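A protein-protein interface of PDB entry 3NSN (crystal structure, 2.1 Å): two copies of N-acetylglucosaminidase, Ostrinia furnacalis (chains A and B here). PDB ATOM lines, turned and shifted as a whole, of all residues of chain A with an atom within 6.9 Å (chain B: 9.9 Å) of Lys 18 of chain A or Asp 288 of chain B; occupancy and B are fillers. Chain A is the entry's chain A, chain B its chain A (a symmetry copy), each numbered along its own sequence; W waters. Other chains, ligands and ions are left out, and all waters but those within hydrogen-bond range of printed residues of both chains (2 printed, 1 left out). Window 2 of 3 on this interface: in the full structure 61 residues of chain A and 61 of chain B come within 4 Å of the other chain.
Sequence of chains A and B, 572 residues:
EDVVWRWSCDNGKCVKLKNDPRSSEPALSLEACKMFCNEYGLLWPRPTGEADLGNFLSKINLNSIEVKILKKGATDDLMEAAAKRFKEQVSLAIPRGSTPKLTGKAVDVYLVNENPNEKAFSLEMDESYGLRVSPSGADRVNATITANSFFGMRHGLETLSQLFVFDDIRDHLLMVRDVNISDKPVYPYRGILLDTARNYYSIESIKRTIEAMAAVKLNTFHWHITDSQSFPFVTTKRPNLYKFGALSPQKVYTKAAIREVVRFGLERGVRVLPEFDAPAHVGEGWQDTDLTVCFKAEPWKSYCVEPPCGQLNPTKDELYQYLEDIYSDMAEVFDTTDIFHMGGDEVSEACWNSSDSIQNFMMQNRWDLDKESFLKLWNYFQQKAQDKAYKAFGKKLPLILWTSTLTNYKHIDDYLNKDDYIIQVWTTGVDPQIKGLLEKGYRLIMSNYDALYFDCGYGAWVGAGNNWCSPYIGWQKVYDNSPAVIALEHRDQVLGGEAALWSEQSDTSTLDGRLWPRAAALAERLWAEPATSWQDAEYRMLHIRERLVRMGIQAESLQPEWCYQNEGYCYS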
ATOM      1  N   VAL A   4       6.751   8.984  -7.698  1.00  0.00           N
ATOM      2  CA  VAL A   4       6.620   7.570  -7.629  1.00  0.00           C
ATOM      3  C   VAL A   4       7.513   6.859  -6.647  1.00  0.00           C
ATOM      4  O   VAL A   4       7.318   5.715  -6.407  1.00  0.00           O
ATOM      5  CB  VAL A   4       6.964   7.091  -9.057  1.00  0.00           C
ATOM      6  CG1 VAL A   4       7.572   5.816  -9.061  1.00  0.00           C
ATOM      7  CG2 VAL A   4       5.760   7.100  -9.898  1.00  0.00           C
ATOM      8  N   TRP A   5       8.503   7.544  -6.110  1.00  0.00           N
ATOM      9  CA  TRP A   5       9.530   6.959  -5.297  1.00  0.00           C
ATOM     10  C   TRP A   5       9.504   7.490  -3.859  1.00  0.00           C
ATOM     11  O   TRP A   5       8.923   8.475  -3.581  1.00  0.00           O
ATOM     12  CB  TRP A   5      10.939   7.169  -5.900  1.00  0.00           C
ATOM     13  CG  TRP A   5      11.163   6.646  -7.291  1.00  0.00           C
ATOM     14  CD1 TRP A   5      11.119   7.341  -8.431  1.00  0.00           C
ATOM     15  CD2 TRP A   5      11.470   5.318  -7.661  1.00  0.00           C
ATOM     16  NE1 TRP A   5      11.352   6.554  -9.482  1.00  0.00           N
ATOM     17  CE2 TRP A   5      11.582   5.293  -9.043  1.00  0.00           C
ATOM     18  CE3 TRP A   5      11.656   4.140  -6.958  1.00  0.00           C
ATOM     19  CZ2 TRP A   5      11.878   4.148  -9.735  1.00  0.00           C
ATOM     20  CZ3 TRP A   5      11.942   3.003  -7.649  1.00  0.00           C
ATOM     21  CH2 TRP A   5      12.051   3.015  -9.022  1.00  0.00           C
ATOM     22  N   ARG A   6      10.178   6.789  -2.984  1.00  0.00           N
ATOM     23  CA  ARG A   6      10.352   7.176  -1.610  1.00  0.00           C
ATOM     24  C   ARG A   6      11.763   6.849  -1.213  1.00  0.00           C
ATOM     25  O   ARG A   6      12.414   6.142  -1.902  1.00  0.00           O
ATOM     26  CB  ARG A   6       9.340   6.492  -0.696  1.00  0.00           C
ATOM     27  CG  ARG A   6       9.629   5.062  -0.413  1.00  0.00           C
ATOM     28  CD  ARG A   6       8.613   4.419   0.484  1.00  0.00           C
ATOM     29  NE  ARG A   6       8.801   2.999   0.593  1.00  0.00           N
ATOM     30  CZ  ARG A   6       9.639   2.420   1.414  1.00  0.00           C
ATOM     31  NH1 ARG A   6      10.356   3.148   2.215  1.00  0.00           N
ATOM     32  NH2 ARG A   6       9.746   1.112   1.455  1.00  0.00           N
ATOM     33  N   VAL A  15      18.248   5.722   0.394  1.00  0.00           N
ATOM     34  CA  VAL A  15      18.079   4.841  -0.741  1.00  0.00           C
ATOM     35  C   VAL A  15      16.712   4.891  -1.352  1.00  0.00           C
ATOM     36  O   VAL A  15      15.749   4.827  -0.677  1.00  0.00           O
ATOM     37  CB  VAL A  15      18.546   3.369  -0.474  1.00  0.00           C
ATOM     38  CG1 VAL A  15      19.233   3.209   0.807  1.00  0.00           C
ATOM     39  CG2 VAL A  15      17.480   2.402  -0.672  1.00  0.00           C
ATOM     40  N   LYS A  16      16.666   5.007  -2.661  1.00  0.00           N
ATOM     41  CA  LYS A  16      15.439   5.160  -3.366  1.00  0.00           C
ATOM     42  C   LYS A  16      14.749   3.824  -3.449  1.00  0.00           C
ATOM     43  O   LYS A  16      15.308   2.879  -3.877  1.00  0.00           O
ATOM     44  CB  LYS A  16      15.674   5.751  -4.767  1.00  0.00           C
ATOM     45  CG  LYS A  16      14.459   6.336  -5.389  1.00  0.00           C
ATOM     46  CD  LYS A  16      14.698   6.964  -6.709  1.00  0.00           C
ATOM     47  CE  LYS A  16      14.888   5.980  -7.812  1.00  0.00           C
ATOM     48  NZ  LYS A  16      14.716   6.515  -9.135  1.00  0.00           N
ATOM     49  N   LEU A  17      13.505   3.810  -3.024  1.00  0.00           N
ATOM     50  CA  LEU A  17      12.680   2.625  -2.985  1.00  0.00           C
ATOM     51  C   LEU A  17      11.331   2.899  -3.556  1.00  0.00           C
ATOM     52  O   LEU A  17      10.842   3.979  -3.504  1.00  0.00           O
ATOM     53  CB  LEU A  17      12.585   2.085  -1.561  1.00  0.00           C
ATOM     54  CG  LEU A  17      13.867   1.558  -0.952  1.00  0.00           C
ATOM     55  CD1 LEU A  17      13.793   1.395   0.523  1.00  0.00           C
ATOM     56  CD2 LEU A  17      14.177   0.280  -1.581  1.00  0.00           C
ATOM     57  N   LYS A  18      10.735   1.908  -4.160  1.00  0.00           N
ATOM     58  CA  LYS A  18       9.455   2.132  -4.749  1.00  0.00           C
ATOM     59  C   LYS A  18       8.448   2.453  -3.659  1.00  0.00           C
ATOM     60  O   LYS A  18       8.501   1.879  -2.626  1.00  0.00           O
ATOM     61  CB  LYS A  18       9.042   0.932  -5.560  1.00  0.00           C
ATOM     62  CG  LYS A  18       7.733   1.062  -6.189  1.00  0.00           C
ATOM     63  CD  LYS A  18       7.869   1.418  -7.626  1.00  0.00           C
ATOM     64  CE  LYS A  18       8.650   0.350  -8.391  1.00  0.00           C
ATOM     65  NZ  LYS A  18       8.606   0.565  -9.856  1.00  0.00           N
ATOM     66  N   ASN A  19       7.576   3.421  -3.896  1.00  0.00           N
ATOM     67  CA  ASN A  19       6.555   3.766  -2.938  1.00  0.00           C
ATOM     68  C   ASN A  19       5.317   2.919  -3.143  1.00  0.00           C
ATOM     69  O   ASN A  19       4.351   3.350  -3.708  1.00  0.00           O
ATOM     70  CB  ASN A  19       6.191   5.230  -2.997  1.00  0.00           C
ATOM     71  CG  ASN A  19       5.313   5.653  -1.853  1.00  0.00           C
ATOM     72  OD1 ASN A  19       4.737   6.681  -1.877  1.00  0.00           O
ATOM     73  ND2 ASN A  19       5.219   4.844  -0.871  1.00  0.00           N
ATOM     74  N   ASP A  20       5.409   1.688  -2.703  1.00  0.00           N
ATOM     75  CA  ASP A  20       4.370   0.691  -2.883  1.00  0.00           C
ATOM     76  C   ASP A  20       3.189   0.943  -1.976  1.00  0.00           C
ATOM     77  O   ASP A  20       3.352   1.181  -0.834  1.00  0.00           O
ATOM     78  CB  ASP A  20       4.963  -0.703  -2.677  1.00  0.00           C
ATOM     79  CG  ASP A  20       5.790  -1.186  -3.862  1.00  0.00           C
ATOM     80  OD1 ASP A  20       6.802  -1.848  -3.632  1.00  0.00           O
ATOM     81  OD2 ASP A  20       5.435  -0.924  -5.032  1.00  0.00           O
ATOM     82  N   PRO A  21       1.989   0.846  -2.502  1.00  0.00           N
ATOM     83  CA  PRO A  21       0.766   1.104  -1.738  1.00  0.00           C
ATOM     84  C   PRO A  21       0.457   0.193  -0.550  1.00  0.00           C
ATOM     85  O   PRO A  21      -0.155   0.624   0.380  1.00  0.00           O
ATOM     86  CB  PRO A  21      -0.316   1.046  -2.799  1.00  0.00           C
ATOM     87  CG  PRO A  21       0.218   0.269  -3.825  1.00  0.00           C
ATOM     88  CD  PRO A  21       1.665   0.474  -3.874  1.00  0.00           C
ATOM     89  N   ASN B 240       5.369   3.565 -18.120  1.00  0.00           N
ATOM     90  CA  ASN B 240       6.135   3.341 -16.930  1.00  0.00           C
ATOM     91  C   ASN B 240       7.633   3.734 -17.081  1.00  0.00           C
ATOM     92  O   ASN B 240       8.277   4.060 -16.118  1.00  0.00           O
ATOM     93  CB  ASN B 240       5.975   1.919 -16.433  1.00  0.00           C
ATOM     94  CG  ASN B 240       4.720   1.716 -15.587  1.00  0.00           C
ATOM     95  OD1 ASN B 240       3.902   2.587 -15.417  1.00  0.00           O
ATOM     96  ND2 ASN B 240       4.585   0.544 -15.068  1.00  0.00           N
ATOM     97  N   LEU B 241       8.152   3.688 -18.291  1.00  0.00           N
ATOM     98  CA  LEU B 241       9.538   3.975 -18.473  1.00  0.00           C
ATOM     99  C   LEU B 241       9.812   5.371 -18.038  1.00  0.00           C
ATOM    100  O   LEU B 241      10.695   5.564 -17.305  1.00  0.00           O
ATOM    101  CB  LEU B 241       9.984   3.773 -19.907  1.00  0.00           C
ATOM    102  CG  LEU B 241       9.823   2.385 -20.495  1.00  0.00           C
ATOM    103  CD1 LEU B 241       9.957   2.451 -21.972  1.00  0.00           C
ATOM    104  CD2 LEU B 241      10.807   1.488 -19.932  1.00  0.00           C
ATOM    105  N   LYS B 243       7.640   7.220 -16.172  1.00  0.00           N
ATOM    106  CA  LYS B 243       7.143   7.374 -14.844  1.00  0.00           C
ATOM    107  C   LYS B 243       8.105   6.919 -13.820  1.00  0.00           C
ATOM    108  O   LYS B 243       8.335   7.607 -12.916  1.00  0.00           O
ATOM    109  CB  LYS B 243       5.828   6.656 -14.655  1.00  0.00           C
ATOM    110  CG  LYS B 243       4.683   7.381 -15.223  1.00  0.00           C
ATOM    111  CD  LYS B 243       3.478   6.525 -15.281  1.00  0.00           C
ATOM    112  CE  LYS B 243       2.217   7.301 -15.156  1.00  0.00           C
ATOM    113  NZ  LYS B 243       1.755   7.944 -16.391  1.00  0.00           N
ATOM    114  N   PHE B 244       8.648   5.735 -13.955  1.00  0.00           N
ATOM    115  CA  PHE B 244       9.737   5.312 -13.123  1.00  0.00           C
ATOM    116  C   PHE B 244      11.082   6.014 -13.392  1.00  0.00           C
ATOM    117  O   PHE B 244      11.853   6.173 -12.506  1.00  0.00           O
ATOM    118  CB  PHE B 244       9.921   3.816 -13.125  1.00  0.00           C
ATOM    119  CG  PHE B 244       8.712   3.066 -12.765  1.00  0.00           C
ATOM    120  CD1 PHE B 244       8.563   1.785 -13.165  1.00  0.00           C
ATOM    121  CD2 PHE B 244       7.707   3.643 -12.053  1.00  0.00           C
ATOM    122  CE1 PHE B 244       7.459   1.088 -12.854  1.00  0.00           C
ATOM    123  CE2 PHE B 244       6.589   2.958 -11.747  1.00  0.00           C
ATOM    124  CZ  PHE B 244       6.464   1.677 -12.137  1.00  0.00           C
ATOM    125  N   GLY B 245      11.347   6.287 -14.661  1.00  0.00           N
ATOM    126  CA  GLY B 245      12.567   6.842 -15.178  1.00  0.00           C
ATOM    127  C   GLY B 245      12.983   8.267 -14.902  1.00  0.00           C
ATOM    128  O   GLY B 245      14.133   8.567 -14.768  1.00  0.00           O
ATOM    129  N   GLY B 283      18.851   1.917 -17.653  1.00  0.00           N
ATOM    130  CA  GLY B 283      18.744   1.711 -16.244  1.00  0.00           C
ATOM    131  C   GLY B 283      17.396   2.109 -15.754  1.00  0.00           C
ATOM    132  O   GLY B 283      16.416   1.396 -15.890  1.00  0.00           O
ATOM    133  N   GLU B 284      17.367   3.349 -15.266  1.00  0.00           N
ATOM    134  CA  GLU B 284      16.188   3.920 -14.720  1.00  0.00           C
ATOM    135  C   GLU B 284      15.054   3.887 -15.711  1.00  0.00           C
ATOM    136  O   GLU B 284      15.185   4.252 -16.801  1.00  0.00           O
ATOM    137  CB  GLU B 284      16.432   5.354 -14.282  1.00  0.00           C
ATOM    138  CG  GLU B 284      17.157   5.498 -13.003  1.00  0.00           C
ATOM    139  CD  GLU B 284      16.374   5.070 -11.784  1.00  0.00           C
ATOM    140  OE1 GLU B 284      17.012   4.828 -10.809  1.00  0.00           O
ATOM    141  OE2 GLU B 284      15.171   4.998 -11.808  1.00  0.00           O
ATOM    142  N   GLY B 285      13.908   3.476 -15.231  1.00  0.00           N
ATOM    143  CA  GLY B 285      12.723   3.358 -16.007  1.00  0.00           C
ATOM    144  C   GLY B 285      12.417   1.943 -16.352  1.00  0.00           C
ATOM    145  O   GLY B 285      11.293   1.647 -16.504  1.00  0.00           O
ATOM    146  N   TRP B 286      13.407   1.084 -16.382  1.00  0.00           N
ATOM    147  CA  TRP B 286      13.248  -0.322 -16.733  1.00  0.00           C
ATOM    148  C   TRP B 286      12.912  -1.301 -15.574  1.00  0.00           C
ATOM    149  O   TRP B 286      12.763  -2.484 -15.771  1.00  0.00           O
ATOM    150  CB  TRP B 286      14.440  -0.796 -17.602  1.00  0.00           C
ATOM    151  CG  TRP B 286      14.547  -0.119 -18.903  1.00  0.00           C
ATOM    152  CD1 TRP B 286      15.155   1.060 -19.165  1.00  0.00           C
ATOM    153  CD2 TRP B 286      13.983  -0.550 -20.140  1.00  0.00           C
ATOM    154  NE1 TRP B 286      15.030   1.375 -20.455  1.00  0.00           N
ATOM    155  CE2 TRP B 286      14.315   0.406 -21.089  1.00  0.00           C
ATOM    156  CE3 TRP B 286      13.230  -1.654 -20.536  1.00  0.00           C
ATOM    157  CZ2 TRP B 286      13.931   0.295 -22.385  1.00  0.00           C
ATOM    158  CZ3 TRP B 286      12.869  -1.755 -21.828  1.00  0.00           C
ATOM    159  CH2 TRP B 286      13.203  -0.793 -22.734  1.00  0.00           C
ATOM    160  N   GLN B 287      12.793  -0.766 -14.378  1.00  0.00           N
ATOM    161  CA  GLN B 287      12.524  -1.537 -13.209  1.00  0.00           C
ATOM    162  C   GLN B 287      11.212  -2.288 -13.324  1.00  0.00           C
ATOM    163  O   GLN B 287      10.256  -1.787 -13.824  1.00  0.00           O
ATOM    164  CB  GLN B 287      12.460  -0.644 -11.961  1.00  0.00           C
ATOM    165  CG  GLN B 287      13.740   0.006 -11.590  1.00  0.00           C
ATOM    166  CD  GLN B 287      13.845   1.454 -12.018  1.00  0.00           C
ATOM    167  OE1 GLN B 287      14.472   2.205 -11.362  1.00  0.00           O
ATOM    168  NE2 GLN B 287      13.248   1.813 -13.095  1.00  0.00           N
ATOM    169  N   ASP B 288      11.249  -3.526 -12.898  1.00  0.00           N
ATOM    170  CA  ASP B 288      10.104  -4.424 -12.929  1.00  0.00           C
ATOM    171  C   ASP B 288       9.801  -4.991 -14.322  1.00  0.00           C
ATOM    172  O   ASP B 288       8.783  -5.568 -14.527  1.00  0.00           O
ATOM    173  CB  ASP B 288       8.829  -3.738 -12.435  1.00  0.00           C
ATOM    174  CG  ASP B 288       8.897  -3.246 -10.979  1.00  0.00           C
ATOM    175  OD1 ASP B 288       9.557  -3.825 -10.121  1.00  0.00           O
ATOM    176  OD2 ASP B 288       8.230  -2.254 -10.710  1.00  0.00           O
ATOM    177  N   THR B 289      10.629  -4.742 -15.296  1.00  0.00           N
ATOM    178  CA  THR B 289      10.357  -5.302 -16.585  1.00  0.00           C
ATOM    179  C   THR B 289      11.048  -6.600 -16.727  1.00  0.00           C
ATOM    180  O   THR B 289      10.680  -7.414 -17.512  1.00  0.00           O
ATOM    181  CB  THR B 289      10.802  -4.436 -17.720  1.00  0.00           C
ATOM    182  OG1 THR B 289      12.223  -4.322 -17.733  1.00  0.00           O
ATOM    183  CG2 THR B 289      10.144  -3.128 -17.638  1.00  0.00           C
ATOM    184  N   ASP B 290      12.107  -6.740 -15.982  1.00  0.00           N
ATOM    185  CA  ASP B 290      13.017  -7.827 -16.149  1.00  0.00           C
ATOM    186  C   ASP B 290      13.740  -7.816 -17.510  1.00  0.00           C
ATOM    187  O   ASP B 290      14.178  -8.836 -17.955  1.00  0.00           O
ATOM    188  CB  ASP B 290      12.287  -9.137 -15.966  1.00  0.00           C
ATOM    189  CG  ASP B 290      13.188 -10.225 -15.528  1.00  0.00           C
ATOM    190  OD1 ASP B 290      13.177 -11.259 -16.172  1.00  0.00           O
ATOM    191  OD2 ASP B 290      13.926 -10.070 -14.549  1.00  0.00           O
ATOM    192  N   LEU B 291      13.827  -6.670 -18.163  1.00  0.00           N
ATOM    193  CA  LEU B 291      14.473  -6.544 -19.455  1.00  0.00           C
ATOM    194  C   LEU B 291      15.919  -6.011 -19.427  1.00  0.00           C
ATOM    195  O   LEU B 291      16.534  -5.885 -20.432  1.00  0.00           O
ATOM    196  CB  LEU B 291      13.604  -5.745 -20.401  1.00  0.00           C
ATOM    197  CG  LEU B 291      12.178  -6.226 -20.640  1.00  0.00           C
ATOM    198  CD1 LEU B 291      11.428  -5.224 -21.357  1.00  0.00           C
ATOM    199  CD2 LEU B 291      12.152  -7.501 -21.409  1.00  0.00           C
ATOM    200  N   THR B 292      16.427  -5.718 -18.250  1.00  0.00           N
ATOM    201  CA  THR B 292      17.771  -5.235 -18.086  1.00  0.00           C
ATOM    202  C   THR B 292      18.523  -6.143 -17.167  1.00  0.00           C
ATOM    203  O   THR B 292      17.947  -6.908 -16.474  1.00  0.00           O
ATOM    204  CB  THR B 292      17.855  -3.835 -17.490  1.00  0.00           C
ATOM    205  OG1 THR B 292      17.192  -3.804 -16.228  1.00  0.00           O
ATOM    206  CG2 THR B 292      17.278  -2.819 -18.417  1.00  0.00           C
ATOM    207  N   PHE B 295      21.567  -3.415 -13.491  1.00  0.00           N
ATOM    208  CA  PHE B 295      21.260  -2.072 -13.127  1.00  0.00           C
ATOM    209  C   PHE B 295      21.832  -1.851 -11.744  1.00  0.00           C
ATOM    210  O   PHE B 295      21.609  -2.604 -10.878  1.00  0.00           O
ATOM    211  CB  PHE B 295      19.768  -1.831 -13.136  1.00  0.00           C
ATOM    212  CG  PHE B 295      19.377  -0.448 -12.749  1.00  0.00           C
ATOM    213  CD1 PHE B 295      20.085   0.628 -13.192  1.00  0.00           C
ATOM    214  CD2 PHE B 295      18.283  -0.208 -11.975  1.00  0.00           C
ATOM    215  CE1 PHE B 295      19.748   1.888 -12.837  1.00  0.00           C
ATOM    216  CE2 PHE B 295      17.944   1.067 -11.653  1.00  0.00           C
ATOM    217  CZ  PHE B 295      18.681   2.107 -12.090  1.00  0.00           C
ATOM    218  N   LYS B 296      22.609  -0.812 -11.556  1.00  0.00           N
ATOM    219  CA  LYS B 296      23.182  -0.503 -10.259  1.00  0.00           C
ATOM    220  C   LYS B 296      24.086  -1.586  -9.728  1.00  0.00           C
ATOM    221  O   LYS B 296      24.290  -1.686  -8.568  1.00  0.00           O
ATOM    222  CB  LYS B 296      22.120  -0.181  -9.240  1.00  0.00           C
ATOM    223  CG  LYS B 296      21.560   1.102  -9.467  1.00  0.00           C
ATOM    224  CD  LYS B 296      20.173   1.134  -9.115  1.00  0.00           C
ATOM    225  CE  LYS B 296      20.010   1.416  -7.745  1.00  0.00           C
ATOM    226  NZ  LYS B 296      18.653   1.130  -7.400  1.00  0.00           N
ATOM    227  N   GLU B 318      10.283  -9.945 -25.452  1.00  0.00           N
ATOM    228  CA  GLU B 318       9.426  -8.824 -25.163  1.00  0.00           C
ATOM    229  C   GLU B 318      10.182  -7.531 -25.350  1.00  0.00           C
ATOM    230  O   GLU B 318       9.598  -6.534 -25.633  1.00  0.00           O
ATOM    231  CB  GLU B 318       8.936  -8.910 -23.747  1.00  0.00           C
ATOM    232  CG  GLU B 318       7.748  -8.083 -23.429  1.00  0.00           C
ATOM    233  CD  GLU B 318       7.502  -8.089 -21.963  1.00  0.00           C
ATOM    234  OE1 GLU B 318       6.617  -7.412 -21.489  1.00  0.00           O
ATOM    235  OE2 GLU B 318       8.217  -8.801 -21.280  1.00  0.00           O
ATOM    236  N   TYR B 322       8.967  -3.552 -26.636  1.00  0.00           N
ATOM    237  CA  TYR B 322       9.209  -2.278 -25.993  1.00  0.00           C
ATOM    238  C   TYR B 322       9.956  -1.275 -26.895  1.00  0.00           C
ATOM    239  O   TYR B 322       9.603  -0.141 -26.991  1.00  0.00           O
ATOM    240  CB  TYR B 322      10.011  -2.484 -24.728  1.00  0.00           C
ATOM    241  CG  TYR B 322       9.259  -2.647 -23.454  1.00  0.00           C
ATOM    242  CD1 TYR B 322       9.245  -1.654 -22.507  1.00  0.00           C
ATOM    243  CD2 TYR B 322       8.619  -3.822 -23.154  1.00  0.00           C
ATOM    244  CE1 TYR B 322       8.594  -1.813 -21.345  1.00  0.00           C
ATOM    245  CE2 TYR B 322       7.966  -3.990 -21.979  1.00  0.00           C
ATOM    246  CZ  TYR B 322       7.947  -2.989 -21.077  1.00  0.00           C
ATOM    247  OH  TYR B 322       7.303  -3.153 -19.924  1.00  0.00           O
HETATM  248  O   HOH W   1      18.087   2.166  -4.552  1.00  0.00           O
HETATM  249  O   HOH W   2      10.548   8.877 -11.307  1.00  0.00           O
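The backbone carbonyl oxygen of Phe 244 of chain B is in hydrogen-bond range of the indole nitrogen of Trp 5 of chain A (3.1 Å).
The side-chain amino group (NZ) of Lys 16 of chain A is in salt-bridge range of the side-chain carboxylate (OE2) of Glu 284 of chain B (3.1 Å).
The side-chain amino group of Lys 18 of chain A lies within salt-bridge range of the side-chain carboxylate of Asp 288 of chain B, 3.0 Å away.
The backbone NH (N) of Asn 19 of chain A is in hydrogen-bond range of the backbone carbonyl oxygen (O) of Val 4 of chain A, 3.4 Å away.
O of Lys 18 of chain A is in hydrogen-bond range of NE of Arg 6 of chain A (3.4 Å).
The side-chain amide oxygen of Gln 287 of chain B sits close to the side-chain carboxylate of Glu 284 of chain B (2.9 Å).
The backbone NH (N) of Gly 285 of chain B lies close to the side-chain amide nitrogen (NE2) of Gln 287 of chain B (2.8 Å).
Among the printed residues, merely in contact across the chains: Val 4 of chain A with Lys 243 of chain B (3.999 Å), Val 4 of chain A with Phe 244 of chain B (3.7 Å), Trp 5 of chain A with Glu 284 of chain B (3.98 Å), Trp 5 of chain A with Gln 287 of chain B (3.5 Å) and Lys 18 of chain A with Phe 244 of chain B (3.3 Å).
Of chain B, only Phe 244 (3.3 Å) and Asp 288 (3.0 Å) come within 4 Å of Lys 18 of chain A.
Of chain A, only Lys 18 comes within 4 Å of Asp 288 of chain B.
No residue of chain B comes within 4 Å of Arg 6 of chain A.
No residue of chain B comes within 4 Å of Leu 17 of chain A.
Of the printed residues of chain A, Glu 284 of chain B touches Trp 5 (3.98 Å) and Lys 16 (3.1 Å).
Of the printed residues of chain B, Lys 16 of chain A touches Glu 284 (3.1 Å).
Of the printed residues of chain A, Phe 244 of chain B touches Val 4, Trp 5 and Lys 18.
Of the printed residues of chain A, Lys 243 of chain B touches Val 4 (3.999 Å).
The nearest residue of chain B that does not touch Lys 18 of chain A is Gln 287 of chain B (4.6 Å).
The nearest residue of chain A that does not touch Asp 288 of chain B is Asp 20 of chain A (6.5 Å).
The nearest printed residue of chain A that does not touch Lys 243 of chain B is Trp 5 of chain A (4.7 Å).
Of the 19 printed residues of chain B, 5 touch a printed residue of chain A.
Of the 10 printed residues of chain A, 4 touch a printed residue of chain B.
Printed residues of chain A that touch a printed residue of chain B: Val 4, Trp 5, Lys 16 and Lys 18.
Hydrophobic or aromatic side chains of chain A within 4 Å of the printed part of chain B: Val 4 and Trp 5.
Among the printed residues, Asp or Glu carboxylates within 4 Å of a Lys or Arg side-chain nitrogen of the other chain: Lys 16 of chain A with Glu 284 of chain B (3.1 Å) and Lys 18 of chain A with Asp 288 of chain B (3.0 Å).
No position is printed for both chains.
Of the 8 pairs that touch across the chains among the printed residues, none has its exchanged pair printed and touching as well.
Water W1 lies within hydrogen-bond range of the backbone carbonyl oxygen (O) of Lys 16 of chain A (2.9 Å) and the side-chain amino group (NZ) of Lys 296 of chain B (3.1 Å).
Water W2 lies within hydrogen-bond range of the backbone carbonyl oxygen (O) of Lys 243 of chain B (3.0 Å), the indole nitrogen (NE1) of Trp 5 of chain A (3.1 Å) and the backbone carbonyl oxygen (O) of Phe 244 of chain B (3.2 Å).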
